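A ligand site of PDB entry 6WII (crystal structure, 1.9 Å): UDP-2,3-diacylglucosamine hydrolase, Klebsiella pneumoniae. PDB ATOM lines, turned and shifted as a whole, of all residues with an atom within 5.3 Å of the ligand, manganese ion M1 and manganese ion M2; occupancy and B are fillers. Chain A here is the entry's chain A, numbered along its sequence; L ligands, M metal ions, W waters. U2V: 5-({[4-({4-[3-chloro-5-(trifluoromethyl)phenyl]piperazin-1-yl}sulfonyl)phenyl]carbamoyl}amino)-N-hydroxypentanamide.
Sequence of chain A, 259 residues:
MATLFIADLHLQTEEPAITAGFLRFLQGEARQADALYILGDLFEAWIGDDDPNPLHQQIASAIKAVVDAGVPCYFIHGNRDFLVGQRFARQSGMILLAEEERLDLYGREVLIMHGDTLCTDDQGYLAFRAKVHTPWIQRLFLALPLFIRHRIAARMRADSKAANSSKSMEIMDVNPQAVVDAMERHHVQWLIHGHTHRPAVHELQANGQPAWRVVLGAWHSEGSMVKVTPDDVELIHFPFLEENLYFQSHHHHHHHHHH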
ATOM      1  N   ASP A   8      -6.918  12.789  -5.817  1.00  0.00           N
ATOM      2  CA  ASP A   8      -8.351  13.006  -5.897  1.00  0.00           C
ATOM      3  C   ASP A   8      -9.086  12.486  -4.653  1.00  0.00           C
ATOM      4  O   ASP A   8     -10.148  11.859  -4.750  1.00  0.00           O
ATOM      5  CB  ASP A   8      -8.914  12.386  -7.168  1.00  0.00           C
ATOM      6  CG  ASP A   8      -8.273  12.982  -8.398  1.00  0.00           C
ATOM      7  OD1 ASP A   8      -8.426  14.207  -8.598  1.00  0.00           O
ATOM      8  OD2 ASP A   8      -7.591  12.256  -9.128  1.00  0.00           O
ATOM      9  N   HIS A  10     -10.053  14.805  -2.407  1.00  0.00           N
ATOM     10  CA  HIS A  10     -10.997  15.909  -2.182  1.00  0.00           C
ATOM     11  C   HIS A  10     -11.435  15.988  -0.726  1.00  0.00           C
ATOM     12  O   HIS A  10     -12.634  16.095  -0.406  1.00  0.00           O
ATOM     13  CB  HIS A  10     -12.219  15.789  -3.102  1.00  0.00           C
ATOM     14  CG  HIS A  10     -11.864  15.770  -4.561  1.00  0.00           C
ATOM     15  ND1 HIS A  10     -11.913  16.895  -5.346  1.00  0.00           N
ATOM     16  CD2 HIS A  10     -11.447  14.762  -5.358  1.00  0.00           C
ATOM     17  CE1 HIS A  10     -11.542  16.586  -6.579  1.00  0.00           C
ATOM     18  NE2 HIS A  10     -11.259  15.295  -6.605  1.00  0.00           N
ATOM     19  N   ASP A  41      -5.319  17.291  -5.868  1.00  0.00           N
ATOM     20  CA  ASP A  41      -6.688  17.214  -5.352  1.00  0.00           C
ATOM     21  C   ASP A  41      -6.720  16.417  -4.067  1.00  0.00           C
ATOM     22  O   ASP A  41      -7.604  15.587  -3.823  1.00  0.00           O
ATOM     23  CB  ASP A  41      -7.660  16.638  -6.394  1.00  0.00           C
ATOM     24  CG  ASP A  41      -7.976  17.631  -7.498  1.00  0.00           C
ATOM     25  OD1 ASP A  41      -7.425  18.764  -7.459  1.00  0.00           O
ATOM     26  OD2 ASP A  41      -8.767  17.294  -8.417  1.00  0.00           O
ATOM     27  N   GLU A  44     -10.441  19.335  -1.241  1.00  0.00           N
ATOM     28  CA  GLU A  44     -11.526  19.806  -2.092  1.00  0.00           C
ATOM     29  C   GLU A  44     -11.362  21.274  -2.444  1.00  0.00           C
ATOM     30  O   GLU A  44     -11.836  21.728  -3.507  1.00  0.00           O
ATOM     31  CB  GLU A  44     -12.866  19.565  -1.393  1.00  0.00           C
ATOM     32  CG  GLU A  44     -14.109  20.176  -2.084  1.00  0.00           C
ATOM     33  CD  GLU A  44     -14.344  19.687  -3.499  1.00  0.00           C
ATOM     34  OE1 GLU A  44     -13.721  18.691  -3.930  1.00  0.00           O
ATOM     35  OE2 GLU A  44     -15.178  20.309  -4.204  1.00  0.00           O
ATOM     36  N   ALA A  45     -10.689  22.039  -1.598  1.00  0.00           N
ATOM     37  CA  ALA A  45     -10.472  23.440  -1.875  1.00  0.00           C
ATOM     38  C   ALA A  45      -9.237  23.880  -1.105  1.00  0.00           C
ATOM     39  O   ALA A  45      -8.850  23.262  -0.117  1.00  0.00           O
ATOM     40  CB  ALA A  45     -11.692  24.277  -1.462  1.00  0.00           C
ATOM     41  N   TRP A  46      -8.630  24.981  -1.560  1.00  0.00           N
ATOM     42  CA  TRP A  46      -7.524  25.565  -0.816  1.00  0.00           C
ATOM     43  C   TRP A  46      -7.474  27.039  -1.153  1.00  0.00           C
ATOM     44  O   TRP A  46      -7.444  27.389  -2.334  1.00  0.00           O
ATOM     45  CB  TRP A  46      -6.178  24.930  -1.188  1.00  0.00           C
ATOM     46  CG  TRP A  46      -5.107  25.152  -0.189  1.00  0.00           C
ATOM     47  CD1 TRP A  46      -4.144  26.130  -0.184  1.00  0.00           C
ATOM     48  CD2 TRP A  46      -4.835  24.320   0.946  1.00  0.00           C
ATOM     49  NE1 TRP A  46      -3.307  25.972   0.916  1.00  0.00           N
ATOM     50  CE2 TRP A  46      -3.715  24.855   1.616  1.00  0.00           C
ATOM     51  CE3 TRP A  46      -5.458  23.182   1.478  1.00  0.00           C
ATOM     52  CZ2 TRP A  46      -3.188  24.277   2.778  1.00  0.00           C
ATOM     53  CZ3 TRP A  46      -4.928  22.607   2.627  1.00  0.00           C
ATOM     54  CH2 TRP A  46      -3.808  23.157   3.262  1.00  0.00           C
ATOM     55  N   ILE A  47      -7.480  27.889  -0.129  1.00  0.00           N
ATOM     56  CA  ILE A  47      -7.424  29.330  -0.366  1.00  0.00           C
ATOM     57  C   ILE A  47      -6.151  29.959   0.186  1.00  0.00           C
ATOM     58  O   ILE A  47      -6.038  31.179   0.230  1.00  0.00           O
ATOM     59  CB  ILE A  47      -8.670  30.043   0.200  1.00  0.00           C
ATOM     60  CG1 ILE A  47      -8.834  29.746   1.701  1.00  0.00           C
ATOM     61  CG2 ILE A  47      -9.904  29.647  -0.582  1.00  0.00           C
ATOM     62  CD1 ILE A  47      -9.888  30.630   2.365  1.00  0.00           C
ATOM     63  N   GLY A  78      -3.239  19.766  -7.688  1.00  0.00           N
ATOM     64  CA  GLY A  78      -4.391  19.496  -8.517  1.00  0.00           C
ATOM     65  C   GLY A  78      -5.081  20.787  -8.931  1.00  0.00           C
ATOM     66  O   GLY A  78      -4.643  21.889  -8.615  1.00  0.00           O
ATOM     67  N   ASN A  79      -6.180  20.624  -9.656  1.00  0.00           N
ATOM     68  CA  ASN A  79      -6.995  21.788 -10.034  1.00  0.00           C
ATOM     69  C   ASN A  79      -7.702  22.399  -8.834  1.00  0.00           C
ATOM     70  O   ASN A  79      -8.026  23.591  -8.862  1.00  0.00           O
ATOM     71  CB  ASN A  79      -7.998  21.407 -11.110  1.00  0.00           C
ATOM     72  CG  ASN A  79      -8.904  20.271 -10.677  1.00  0.00           C
ATOM     73  OD1 ASN A  79      -8.467  19.140 -10.529  1.00  0.00           O
ATOM     74  ND2 ASN A  79     -10.199  20.567 -10.493  1.00  0.00           N
ATOM     75  N   ARG A  80      -7.953  21.620  -7.784  1.00  0.00           N
ATOM     76  CA  ARG A  80      -8.636  22.168  -6.607  1.00  0.00           C
ATOM     77  C   ARG A  80      -7.677  22.812  -5.627  1.00  0.00           C
ATOM     78  O   ARG A  80      -8.052  23.799  -4.966  1.00  0.00           O
ATOM     79  CB  ARG A  80      -9.418  21.080  -5.867  1.00  0.00           C
ATOM     80  CG  ARG A  80     -10.410  20.322  -6.701  1.00  0.00           C
ATOM     81  CD  ARG A  80     -11.468  21.232  -7.306  1.00  0.00           C
ATOM     82  NE  ARG A  80     -12.319  21.788  -6.254  1.00  0.00           N
ATOM     83  CZ  ARG A  80     -13.420  22.486  -6.491  1.00  0.00           C
ATOM     84  NH1 ARG A  80     -13.823  22.703  -7.744  1.00  0.00           N
ATOM     85  NH2 ARG A  80     -14.143  22.960  -5.482  1.00  0.00           N
ATOM     86  N   PHE A  82      -4.307  23.982  -6.049  1.00  0.00           N
ATOM     87  CA  PHE A  82      -3.114  24.572  -6.621  1.00  0.00           C
ATOM     88  C   PHE A  82      -2.483  25.656  -5.739  1.00  0.00           C
ATOM     89  O   PHE A  82      -1.321  26.009  -5.959  1.00  0.00           O
ATOM     90  CB  PHE A  82      -3.445  25.157  -8.013  1.00  0.00           C
ATOM     91  CG  PHE A  82      -4.549  26.198  -7.995  1.00  0.00           C
ATOM     92  CD1 PHE A  82      -5.883  25.826  -8.170  1.00  0.00           C
ATOM     93  CD2 PHE A  82      -4.241  27.549  -7.854  1.00  0.00           C
ATOM     94  CE1 PHE A  82      -6.889  26.774  -8.168  1.00  0.00           C
ATOM     95  CE2 PHE A  82      -5.259  28.503  -7.847  1.00  0.00           C
ATOM     96  CZ  PHE A  82      -6.580  28.122  -8.005  1.00  0.00           C
ATOM     97  N   LEU A  83      -3.190  26.168  -4.740  1.00  0.00           N
ATOM     98  CA  LEU A  83      -2.602  27.164  -3.844  1.00  0.00           C
ATOM     99  C   LEU A  83      -1.854  26.566  -2.663  1.00  0.00           C
ATOM    100  O   LEU A  83      -1.293  27.313  -1.860  1.00  0.00           O
ATOM    101  CB  LEU A  83      -3.671  28.137  -3.322  1.00  0.00           C
ATOM    102  CG  LEU A  83      -4.231  29.071  -4.386  1.00  0.00           C
ATOM    103  CD1 LEU A  83      -5.232  30.041  -3.764  1.00  0.00           C
ATOM    104  CD2 LEU A  83      -3.106  29.818  -5.107  1.00  0.00           C
ATOM    105  N   HIS A 114      -0.851  15.536 -12.297  1.00  0.00           N
ATOM    106  CA  HIS A 114      -2.237  15.463 -11.851  1.00  0.00           C
ATOM    107  C   HIS A 114      -3.143  14.947 -12.952  1.00  0.00           C
ATOM    108  O   HIS A 114      -4.027  14.117 -12.709  1.00  0.00           O
ATOM    109  CB  HIS A 114      -2.745  16.834 -11.366  1.00  0.00           C
ATOM    110  CG  HIS A 114      -4.161  16.784 -10.916  1.00  0.00           C
ATOM    111  ND1 HIS A 114      -4.596  15.936  -9.925  1.00  0.00           N
ATOM    112  CD2 HIS A 114      -5.271  17.443 -11.350  1.00  0.00           C
ATOM    113  CE1 HIS A 114      -5.901  16.093  -9.744  1.00  0.00           C
ATOM    114  NE2 HIS A 114      -6.328  16.998 -10.605  1.00  0.00           N
ATOM    115  N   ASP A 116      -4.889  17.127 -15.286  1.00  0.00           N
ATOM    116  CA  ASP A 116      -5.794  18.104 -15.895  1.00  0.00           C
ATOM    117  C   ASP A 116      -5.180  18.744 -17.123  1.00  0.00           C
ATOM    118  O   ASP A 116      -5.915  19.141 -18.045  1.00  0.00           O
ATOM    119  CB  ASP A 116      -6.202  19.180 -14.878  1.00  0.00           C
ATOM    120  CG  ASP A 116      -5.020  19.938 -14.315  1.00  0.00           C
ATOM    121  OD1 ASP A 116      -4.031  19.306 -13.885  1.00  0.00           O
ATOM    122  OD2 ASP A 116      -5.068  21.178 -14.310  1.00  0.00           O
ATOM    123  N   CYS A 119      -6.160  17.301 -20.553  1.00  0.00           N
ATOM    124  CA  CYS A 119      -7.543  17.403 -20.997  1.00  0.00           C
ATOM    125  C   CYS A 119      -7.703  18.627 -21.896  1.00  0.00           C
ATOM    126  O   CYS A 119      -8.450  19.561 -21.601  1.00  0.00           O
ATOM    127  CB  CYS A 119      -8.472  17.440 -19.789  1.00  0.00           C
ATOM    128  SG  CYS A 119      -8.344  15.944 -18.741  1.00  0.00           S
ATOM    129  N   ASP A 122     -10.914  20.583 -23.239  1.00  0.00           N
ATOM    130  CA  ASP A 122     -11.643  21.556 -22.422  1.00  0.00           C
ATOM    131  C   ASP A 122     -10.889  22.879 -22.473  1.00  0.00           C
ATOM    132  O   ASP A 122     -10.158  23.272 -21.558  1.00  0.00           O
ATOM    133  CB  ASP A 122     -11.823  21.064 -20.998  1.00  0.00           C
ATOM    134  CG  ASP A 122     -12.840  21.892 -20.217  1.00  0.00           C
ATOM    135  OD1 ASP A 122     -13.055  23.068 -20.586  1.00  0.00           O
ATOM    136  OD2 ASP A 122     -13.405  21.374 -19.233  1.00  0.00           O
ATOM    137  N   TYR A 125     -11.557  25.345 -19.551  1.00  0.00           N
ATOM    138  CA  TYR A 125     -10.818  25.055 -18.328  1.00  0.00           C
ATOM    139  C   TYR A 125      -9.365  25.482 -18.445  1.00  0.00           C
ATOM    140  O   TYR A 125      -8.814  26.070 -17.507  1.00  0.00           O
ATOM    141  CB  TYR A 125     -10.877  23.565 -17.974  1.00  0.00           C
ATOM    142  CG  TYR A 125      -9.862  23.253 -16.898  1.00  0.00           C
ATOM    143  CD1 TYR A 125      -9.997  23.799 -15.638  1.00  0.00           C
ATOM    144  CD2 TYR A 125      -8.734  22.494 -17.162  1.00  0.00           C
ATOM    145  CE1 TYR A 125      -9.065  23.557 -14.644  1.00  0.00           C
ATOM    146  CE2 TYR A 125      -7.792  22.246 -16.173  1.00  0.00           C
ATOM    147  CZ  TYR A 125      -7.974  22.779 -14.922  1.00  0.00           C
ATOM    148  OH  TYR A 125      -7.045  22.547 -13.926  1.00  0.00           O
ATOM    149  N   PHE A 128      -9.019  29.141 -17.750  1.00  0.00           N
ATOM    150  CA  PHE A 128      -9.112  29.359 -16.311  1.00  0.00           C
ATOM    151  C   PHE A 128      -7.832  28.916 -15.611  1.00  0.00           C
ATOM    152  O   PHE A 128      -7.275  29.647 -14.782  1.00  0.00           O
ATOM    153  CB  PHE A 128     -10.329  28.617 -15.757  1.00  0.00           C
ATOM    154  CG  PHE A 128     -10.376  28.565 -14.245  1.00  0.00           C
ATOM    155  CD1 PHE A 128     -10.922  29.608 -13.528  1.00  0.00           C
ATOM    156  CD2 PHE A 128      -9.907  27.454 -13.560  1.00  0.00           C
ATOM    157  CE1 PHE A 128     -10.976  29.559 -12.138  1.00  0.00           C
ATOM    158  CE2 PHE A 128      -9.951  27.390 -12.185  1.00  0.00           C
ATOM    159  CZ  PHE A 128     -10.492  28.446 -11.471  1.00  0.00           C
ATOM    160  N   VAL A 132      -5.362  31.157 -13.075  1.00  0.00           N
ATOM    161  CA  VAL A 132      -5.109  30.945 -11.652  1.00  0.00           C
ATOM    162  C   VAL A 132      -3.710  30.406 -11.375  1.00  0.00           C
ATOM    163  O   VAL A 132      -3.305  30.361 -10.218  1.00  0.00           O
ATOM    164  CB  VAL A 132      -6.158  30.027 -10.978  1.00  0.00           C
ATOM    165  CG1 VAL A 132      -7.526  30.660 -11.024  1.00  0.00           C
ATOM    166  CG2 VAL A 132      -6.153  28.616 -11.601  1.00  0.00           C
ATOM    167  N   ILE A 137      -1.321  36.876 -10.255  1.00  0.00           N
ATOM    168  CA  ILE A 137      -2.712  36.694  -9.871  1.00  0.00           C
ATOM    169  C   ILE A 137      -2.821  35.923  -8.558  1.00  0.00           C
ATOM    170  O   ILE A 137      -3.611  36.289  -7.681  1.00  0.00           O
ATOM    171  CB  ILE A 137      -3.501  36.008 -11.009  1.00  0.00           C
ATOM    172  CG1 ILE A 137      -3.588  36.938 -12.222  1.00  0.00           C
ATOM    173  CG2 ILE A 137      -4.886  35.617 -10.543  1.00  0.00           C
ATOM    174  CD1 ILE A 137      -4.358  36.324 -13.382  1.00  0.00           C
ATOM    175  N   GLN A 138      -2.052  34.840  -8.406  1.00  0.00           N
ATOM    176  CA  GLN A 138      -2.061  34.135  -7.125  1.00  0.00           C
ATOM    177  C   GLN A 138      -1.631  35.048  -5.984  1.00  0.00           C
ATOM    178  O   GLN A 138      -2.202  35.010  -4.896  1.00  0.00           O
ATOM    179  CB  GLN A 138      -1.148  32.910  -7.161  1.00  0.00           C
ATOM    180  CG  GLN A 138      -1.507  31.864  -8.177  1.00  0.00           C
ATOM    181  CD  GLN A 138      -0.654  30.627  -8.022  1.00  0.00           C
ATOM    182  OE1 GLN A 138       0.346  30.655  -7.309  1.00  0.00           O
ATOM    183  NE2 GLN A 138      -1.048  29.541  -8.668  1.00  0.00           N
ATOM    184  N   PHE A 141      -4.524  37.301  -5.010  1.00  0.00           N
ATOM    185  CA  PHE A 141      -5.572  36.580  -4.308  1.00  0.00           C
ATOM    186  C   PHE A 141      -5.135  36.256  -2.889  1.00  0.00           C
ATOM    187  O   PHE A 141      -5.881  36.467  -1.930  1.00  0.00           O
ATOM    188  CB  PHE A 141      -5.943  35.305  -5.063  1.00  0.00           C
ATOM    189  CG  PHE A 141      -6.948  34.445  -4.335  1.00  0.00           C
ATOM    190  CD1 PHE A 141      -8.310  34.700  -4.454  1.00  0.00           C
ATOM    191  CD2 PHE A 141      -6.529  33.397  -3.522  1.00  0.00           C
ATOM    192  CE1 PHE A 141      -9.226  33.897  -3.786  1.00  0.00           C
ATOM    193  CE2 PHE A 141      -7.443  32.616  -2.856  1.00  0.00           C
ATOM    194  CZ  PHE A 141      -8.782  32.859  -2.987  1.00  0.00           C
ATOM    195  N   ILE A 152     -15.090  34.336  -1.646  1.00  0.00           N
ATOM    196  CA  ILE A 152     -14.858  34.075  -3.078  1.00  0.00           C
ATOM    197  C   ILE A 152     -14.952  32.588  -3.363  1.00  0.00           C
ATOM    198  O   ILE A 152     -15.636  32.160  -4.302  1.00  0.00           O
ATOM    199  CB  ILE A 152     -13.490  34.635  -3.504  1.00  0.00           C
ATOM    200  CG1 ILE A 152     -13.466  36.161  -3.432  1.00  0.00           C
ATOM    201  CG2 ILE A 152     -13.125  34.158  -4.911  1.00  0.00           C
ATOM    202  CD1 ILE A 152     -12.071  36.717  -3.612  1.00  0.00           C
ATOM    203  N   ALA A 153     -14.290  31.783  -2.550  1.00  0.00           N
ATOM    204  CA  ALA A 153     -14.280  30.340  -2.767  1.00  0.00           C
ATOM    205  C   ALA A 153     -15.679  29.736  -2.629  1.00  0.00           C
ATOM    206  O   ALA A 153     -16.076  28.880  -3.427  1.00  0.00           O
ATOM    207  CB  ALA A 153     -13.308  29.661  -1.806  1.00  0.00           C
ATOM    208  N   MET A 156     -17.659  30.667  -5.758  1.00  0.00           N
ATOM    209  CA  MET A 156     -17.240  29.945  -6.949  1.00  0.00           C
ATOM    210  C   MET A 156     -17.652  28.483  -6.895  1.00  0.00           C
ATOM    211  O   MET A 156     -18.163  27.945  -7.878  1.00  0.00           O
ATOM    212  CB  MET A 156     -15.733  30.059  -7.120  1.00  0.00           C
ATOM    213  CG  MET A 156     -15.268  31.442  -7.484  1.00  0.00           C
ATOM    214  SD  MET A 156     -13.489  31.465  -7.616  1.00  0.00           S
ATOM    215  CE  MET A 156     -13.240  30.165  -8.815  1.00  0.00           C
ATOM    216  N   ARG A 157     -17.442  27.822  -5.754  1.00  0.00           N
ATOM    217  CA  ARG A 157     -17.830  26.422  -5.636  1.00  0.00           C
ATOM    218  C   ARG A 157     -19.328  26.234  -5.830  1.00  0.00           C
ATOM    219  O   ARG A 157     -19.761  25.174  -6.285  1.00  0.00           O
ATOM    220  CB  ARG A 157     -17.396  25.863  -4.277  1.00  0.00           C
ATOM    221  CG  ARG A 157     -15.893  25.680  -4.133  1.00  0.00           C
ATOM    222  CD  ARG A 157     -15.569  24.960  -2.847  1.00  0.00           C
ATOM    223  NE  ARG A 157     -16.104  25.661  -1.685  1.00  0.00           N
ATOM    224  CZ  ARG A 157     -15.380  26.425  -0.878  1.00  0.00           C
ATOM    225  NH1 ARG A 157     -14.086  26.577  -1.107  1.00  0.00           N
ATOM    226  NH2 ARG A 157     -15.954  27.037   0.149  1.00  0.00           N
ATOM    227  N   GLU A 170     -19.663  16.352 -14.893  1.00  0.00           N
ATOM    228  CA  GLU A 170     -18.805  15.389 -15.575  1.00  0.00           C
ATOM    229  C   GLU A 170     -17.430  15.977 -15.881  1.00  0.00           C
ATOM    230  O   GLU A 170     -17.326  17.100 -16.385  1.00  0.00           O
ATOM    231  CB  GLU A 170     -19.472  14.910 -16.873  1.00  0.00           C
ATOM    232  N   ILE A 171     -16.385  15.220 -15.568  1.00  0.00           N
ATOM    233  CA  ILE A 171     -15.013  15.647 -15.790  1.00  0.00           C
ATOM    234  C   ILE A 171     -14.616  15.266 -17.204  1.00  0.00           C
ATOM    235  O   ILE A 171     -14.734  14.092 -17.599  1.00  0.00           O
ATOM    236  CB  ILE A 171     -14.058  15.027 -14.752  1.00  0.00           C
ATOM    237  CG1 ILE A 171     -14.460  15.428 -13.336  1.00  0.00           C
ATOM    238  CG2 ILE A 171     -12.614  15.432 -15.034  1.00  0.00           C
ATOM    239  CD1 ILE A 171     -13.707  14.686 -12.245  1.00  0.00           C
ATOM    240  N   MET A 172     -14.152  16.242 -17.987  1.00  0.00           N
ATOM    241  CA  MET A 172     -13.669  15.960 -19.326  1.00  0.00           C
ATOM    242  C   MET A 172     -12.444  15.048 -19.252  1.00  0.00           C
ATOM    243  O   MET A 172     -11.572  15.240 -18.396  1.00  0.00           O
ATOM    244  CB  MET A 172     -13.314  17.265 -20.059  1.00  0.00           C
ATOM    245  CG  MET A 172     -12.715  17.076 -21.428  1.00  0.00           C
ATOM    246  SD  MET A 172     -13.946  17.061 -22.755  1.00  0.00           S
ATOM    247  CE  MET A 172     -14.487  18.768 -22.715  1.00  0.00           C
ATOM    248  N   ASP A 173     -12.401  14.053 -20.134  1.00  0.00           N
ATOM    249  CA  ASP A 173     -11.328  13.072 -20.125  1.00  0.00           C
ATOM    250  C   ASP A 173     -10.118  13.598 -20.886  1.00  0.00           C
ATOM    251  O   ASP A 173     -10.150  14.673 -21.497  1.00  0.00           O
ATOM    252  CB  ASP A 173     -11.842  11.751 -20.712  1.00  0.00           C
ATOM    253  CG  ASP A 173     -11.032  10.545 -20.262  1.00  0.00           C
ATOM    254  OD1 ASP A 173     -10.006  10.700 -19.566  1.00  0.00           O
ATOM    255  OD2 ASP A 173     -11.439   9.417 -20.628  1.00  0.00           O
ATOM    256  N   HIS A 195      -7.066  13.065 -11.639  1.00  0.00           N
ATOM    257  CA  HIS A 195      -7.964  14.098 -12.174  1.00  0.00           C
ATOM    258  C   HIS A 195      -9.230  13.568 -12.822  1.00  0.00           C
ATOM    259  O   HIS A 195     -10.319  14.094 -12.539  1.00  0.00           O
ATOM    260  CB  HIS A 195      -7.289  15.005 -13.214  1.00  0.00           C
ATOM    261  CG  HIS A 195      -8.179  16.138 -13.620  1.00  0.00           C
ATOM    262  ND1 HIS A 195      -8.578  17.120 -12.741  1.00  0.00           N
ATOM    263  CD2 HIS A 195      -8.830  16.405 -14.787  1.00  0.00           C
ATOM    264  CE1 HIS A 195      -9.387  17.969 -13.352  1.00  0.00           C
ATOM    265  NE2 HIS A 195      -9.566  17.546 -14.595  1.00  0.00           N
ATOM    266  N   HIS A 197     -10.874  10.743 -12.632  1.00  0.00           N
ATOM    267  CA  HIS A 197     -11.767   9.898 -11.839  1.00  0.00           C
ATOM    268  C   HIS A 197     -12.213   8.641 -12.589  1.00  0.00           C
ATOM    269  O   HIS A 197     -13.287   8.110 -12.331  1.00  0.00           O
ATOM    270  CB  HIS A 197     -12.994  10.682 -11.364  1.00  0.00           C
ATOM    271  CG  HIS A 197     -12.679  11.811 -10.439  1.00  0.00           C
ATOM    272  ND1 HIS A 197     -13.647  12.446  -9.679  1.00  0.00           N
ATOM    273  CD2 HIS A 197     -11.503  12.425 -10.141  1.00  0.00           C
ATOM    274  CE1 HIS A 197     -13.074  13.396  -8.955  1.00  0.00           C
ATOM    275  NE2 HIS A 197     -11.776  13.408  -9.228  1.00  0.00           N
HETATM  276  C13 U2V L   1     -10.845  25.338  -6.804  1.00  0.00           C
HETATM  277  C15 U2V L   1     -12.296  25.379  -8.718  1.00  0.00           C
HETATM  278  C17 U2V L   1     -12.844  26.687  -6.782  1.00  0.00           C
HETATM  279  C22 U2V L   1     -11.895  22.608 -13.008  1.00  0.00           C
HETATM  280  C24 U2V L   1     -12.311  20.298 -13.928  1.00  0.00           C
HETATM  281  C26 U2V L   1     -11.709  19.596 -16.248  1.00  0.00           C
HETATM  282  C01 U2V L   1      -7.481  31.562  -6.798  1.00  0.00           C
HETATM  283  C02 U2V L   1      -8.833  31.523  -6.598  1.00  0.00           C
HETATM  284  C04 U2V L   1     -10.680  30.611  -5.204  1.00  0.00           C
HETATM  285  C05 U2V L   1     -11.372  29.263  -5.299  1.00  0.00           C
HETATM  286  C07 U2V L   1      -9.214  28.145  -5.264  1.00  0.00           C
HETATM  287  C08 U2V L   1      -8.522  29.493  -5.169  1.00  0.00           C
HETATM  288  C12 U2V L   1     -11.692  26.215  -6.160  1.00  0.00           C
HETATM  289  C14 U2V L   1     -11.158  24.911  -8.077  1.00  0.00           C
HETATM  290  C16 U2V L   1     -13.127  26.281  -8.072  1.00  0.00           C
HETATM  291  C19 U2V L   1     -12.002  23.931 -10.889  1.00  0.00           C
HETATM  292  C23 U2V L   1     -12.953  21.643 -13.553  1.00  0.00           C
HETATM  293  C25 U2V L   1     -11.340  20.509 -15.086  1.00  0.00           C
HETATM  294  C30 U2V L   1      -9.691  32.490  -7.106  1.00  0.00           C
HETATM  295  C31 U2V L   1      -9.158  33.503  -7.848  1.00  0.00           C
HETATM  296  C32 U2V L   1      -7.797  33.570  -8.077  1.00  0.00           C
HETATM  297  C33 U2V L   1      -6.963  32.593  -7.555  1.00  0.00           C
HETATM  298  C35 U2V L   1     -10.111  34.563  -8.399  1.00  0.00           C
HETATM  299  F36 U2V L   1     -10.721  35.185  -7.364  1.00  0.00           F
HETATM  300  F37 U2V L   1     -11.049  33.949  -9.163  1.00  0.00           F
HETATM  301  F38 U2V L   1      -9.405  35.467  -9.116  1.00  0.00           F
HETATM  302  N03 U2V L   1      -9.384  30.467  -5.812  1.00  0.00           N
HETATM  303  N06 U2V L   1     -10.524  28.245  -4.670  1.00  0.00           N
HETATM  304  N18 U2V L   1     -12.680  24.937 -10.043  1.00  0.00           N
HETATM  305  N21 U2V L   1     -12.556  23.601 -12.183  1.00  0.00           N
HETATM  306  N28 U2V L   1     -10.685  18.794 -16.887  1.00  0.00           N
HETATM  307  O10 U2V L   1     -10.311  25.885  -3.827  1.00  0.00           O
HETATM  308  O11 U2V L   1     -12.486  26.880  -3.691  1.00  0.00           O
HETATM  309  O20 U2V L   1     -11.010  23.378 -10.575  1.00  0.00           O
HETATM  310  O27 U2V L   1     -12.832  19.538 -16.634  1.00  0.00           O
HETATM  311  O29 U2V L   1     -11.024  17.940 -17.954  1.00  0.00           O
HETATM  312  S09 U2V L   1     -11.274  26.759  -4.504  1.00  0.00           S
HETATM  313 CL34 U2V L   1      -5.207  32.594  -7.811  1.00  0.00          CL
HETATM  314 MN    MN M   1      -8.549  17.224 -10.583  1.00  0.00          MN
HETATM  315 MN    MN M   2     -10.262  15.069  -8.593  1.00  0.00          MN
HETATM  316  O   HOH W   1     -11.770  18.084  -9.795  1.00  0.00           O
HETATM  317  O   HOH W   2     -10.289  16.001 -10.224  1.00  0.00           O
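An oxygen (O20) of the ligand is in hydrogen-bond range of the side-chain amide nitrogen of Asn 79 (2.9 Å).
A ring nitrogen (NE2) of His 195 lies within hydrogen-bond range of a nitrogen (N28) of the ligand (2.8 Å).
O of Met 172 lies within hydrogen-bond range of O29 of the ligand.
O10 of the ligand is in hydrogen-bond range of N of Trp 46.
NH1 of Arg 157 is in hydrogen-bond range of O11 of the ligand.
The side-chain sulfur (SG) of Cys 119 lies close to an oxygen (O29) of the ligand (3.4 Å).
OD2 of Asp 8 lies within hydrogen-bond range of N of His 195 (2.7 Å).
OD1 of Asp 41 sits at hydrogen-bond distance from N of Arg 80.
The side-chain carboxylate (OE1) of Glu 44 is in hydrogen-bond range of a ring nitrogen (ND1) of His 10 (2.9 Å).
O of Met 172 is in hydrogen-bond range of SG of Cys 119 (3.3 Å).
The side-chain sulfur (SG) of Cys 119 lies within hydrogen-bond range of the backbone carbonyl oxygen (O) of Asp 173, at 3.5 Å.
OE2 of Glu 44 is in salt-bridge range of NH2 of Arg 80 (3.1 Å).
The side-chain carboxylate (OD1) of Asp 122 sits at hydrogen-bond distance from the backbone NH (N) of Tyr 125.
The side-chain amide nitrogen (NE2) of Gln 138 lies within hydrogen-bond range of the backbone carbonyl oxygen (O) of Val 132.
O10 of the ligand lies close to O of Arg 80 (3.3 Å).
The side-chain carboxylate (OD2) of Asp 122 sits close to an oxygen (O27) of the ligand.
Residues that only touch the ligand: Ala 45, Tyr 125, Ala 153, Gln 138, Ile 152, Leu 83, Phe 141, Phe 82, Val 132 and Met 156.
Within 4 Å of the ligand: Ala 45, Trp 46, Asn 79, Arg 80, Phe 82, Leu 83, Cys 119, Asp 122, Tyr 125, Val 132, Gln 138, Phe 141, Ile 152, Ala 153, Met 156, Arg 157, Met 172 and His 195.
Five residues have an atom within 4 Å of manganese ion M1: Asp 8, Asp 41, Asn 79, His 114 and His 195.
The nearest printed residue that does not touch manganese ion M1 is His 10 (5.0 Å).
Within 4 Å of manganese ion M2: Asp 8, His 10, Asp 41 and His 197.
The nearest printed residue that does not touch manganese ion M2 is His 195 (4.1 Å).
OD1 of Asn 79 binds manganese ion M1 (1.9 Å).
Water W2 is bound to manganese ion M1 (2.2 Å).
A ring nitrogen (ND1) of His 195 is bound to manganese ion M1, at 2.2 Å.
The side-chain carboxylate (OD2) of Asp 41 binds manganese ion M1, 2.2 Å away.
Manganese ion M1 is bound by NE2 of His 114.
Manganese ion M2 is bound by water W2 (1.9 Å), OD1 of Asp 8 (2.0 Å), NE2 of His 10 (2.2 Å), NE2 of His 197 (2.3 Å) and OD2 of Asp 41 (2.7 Å).
Manganese ion M2 has five donor atoms within binding distance.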
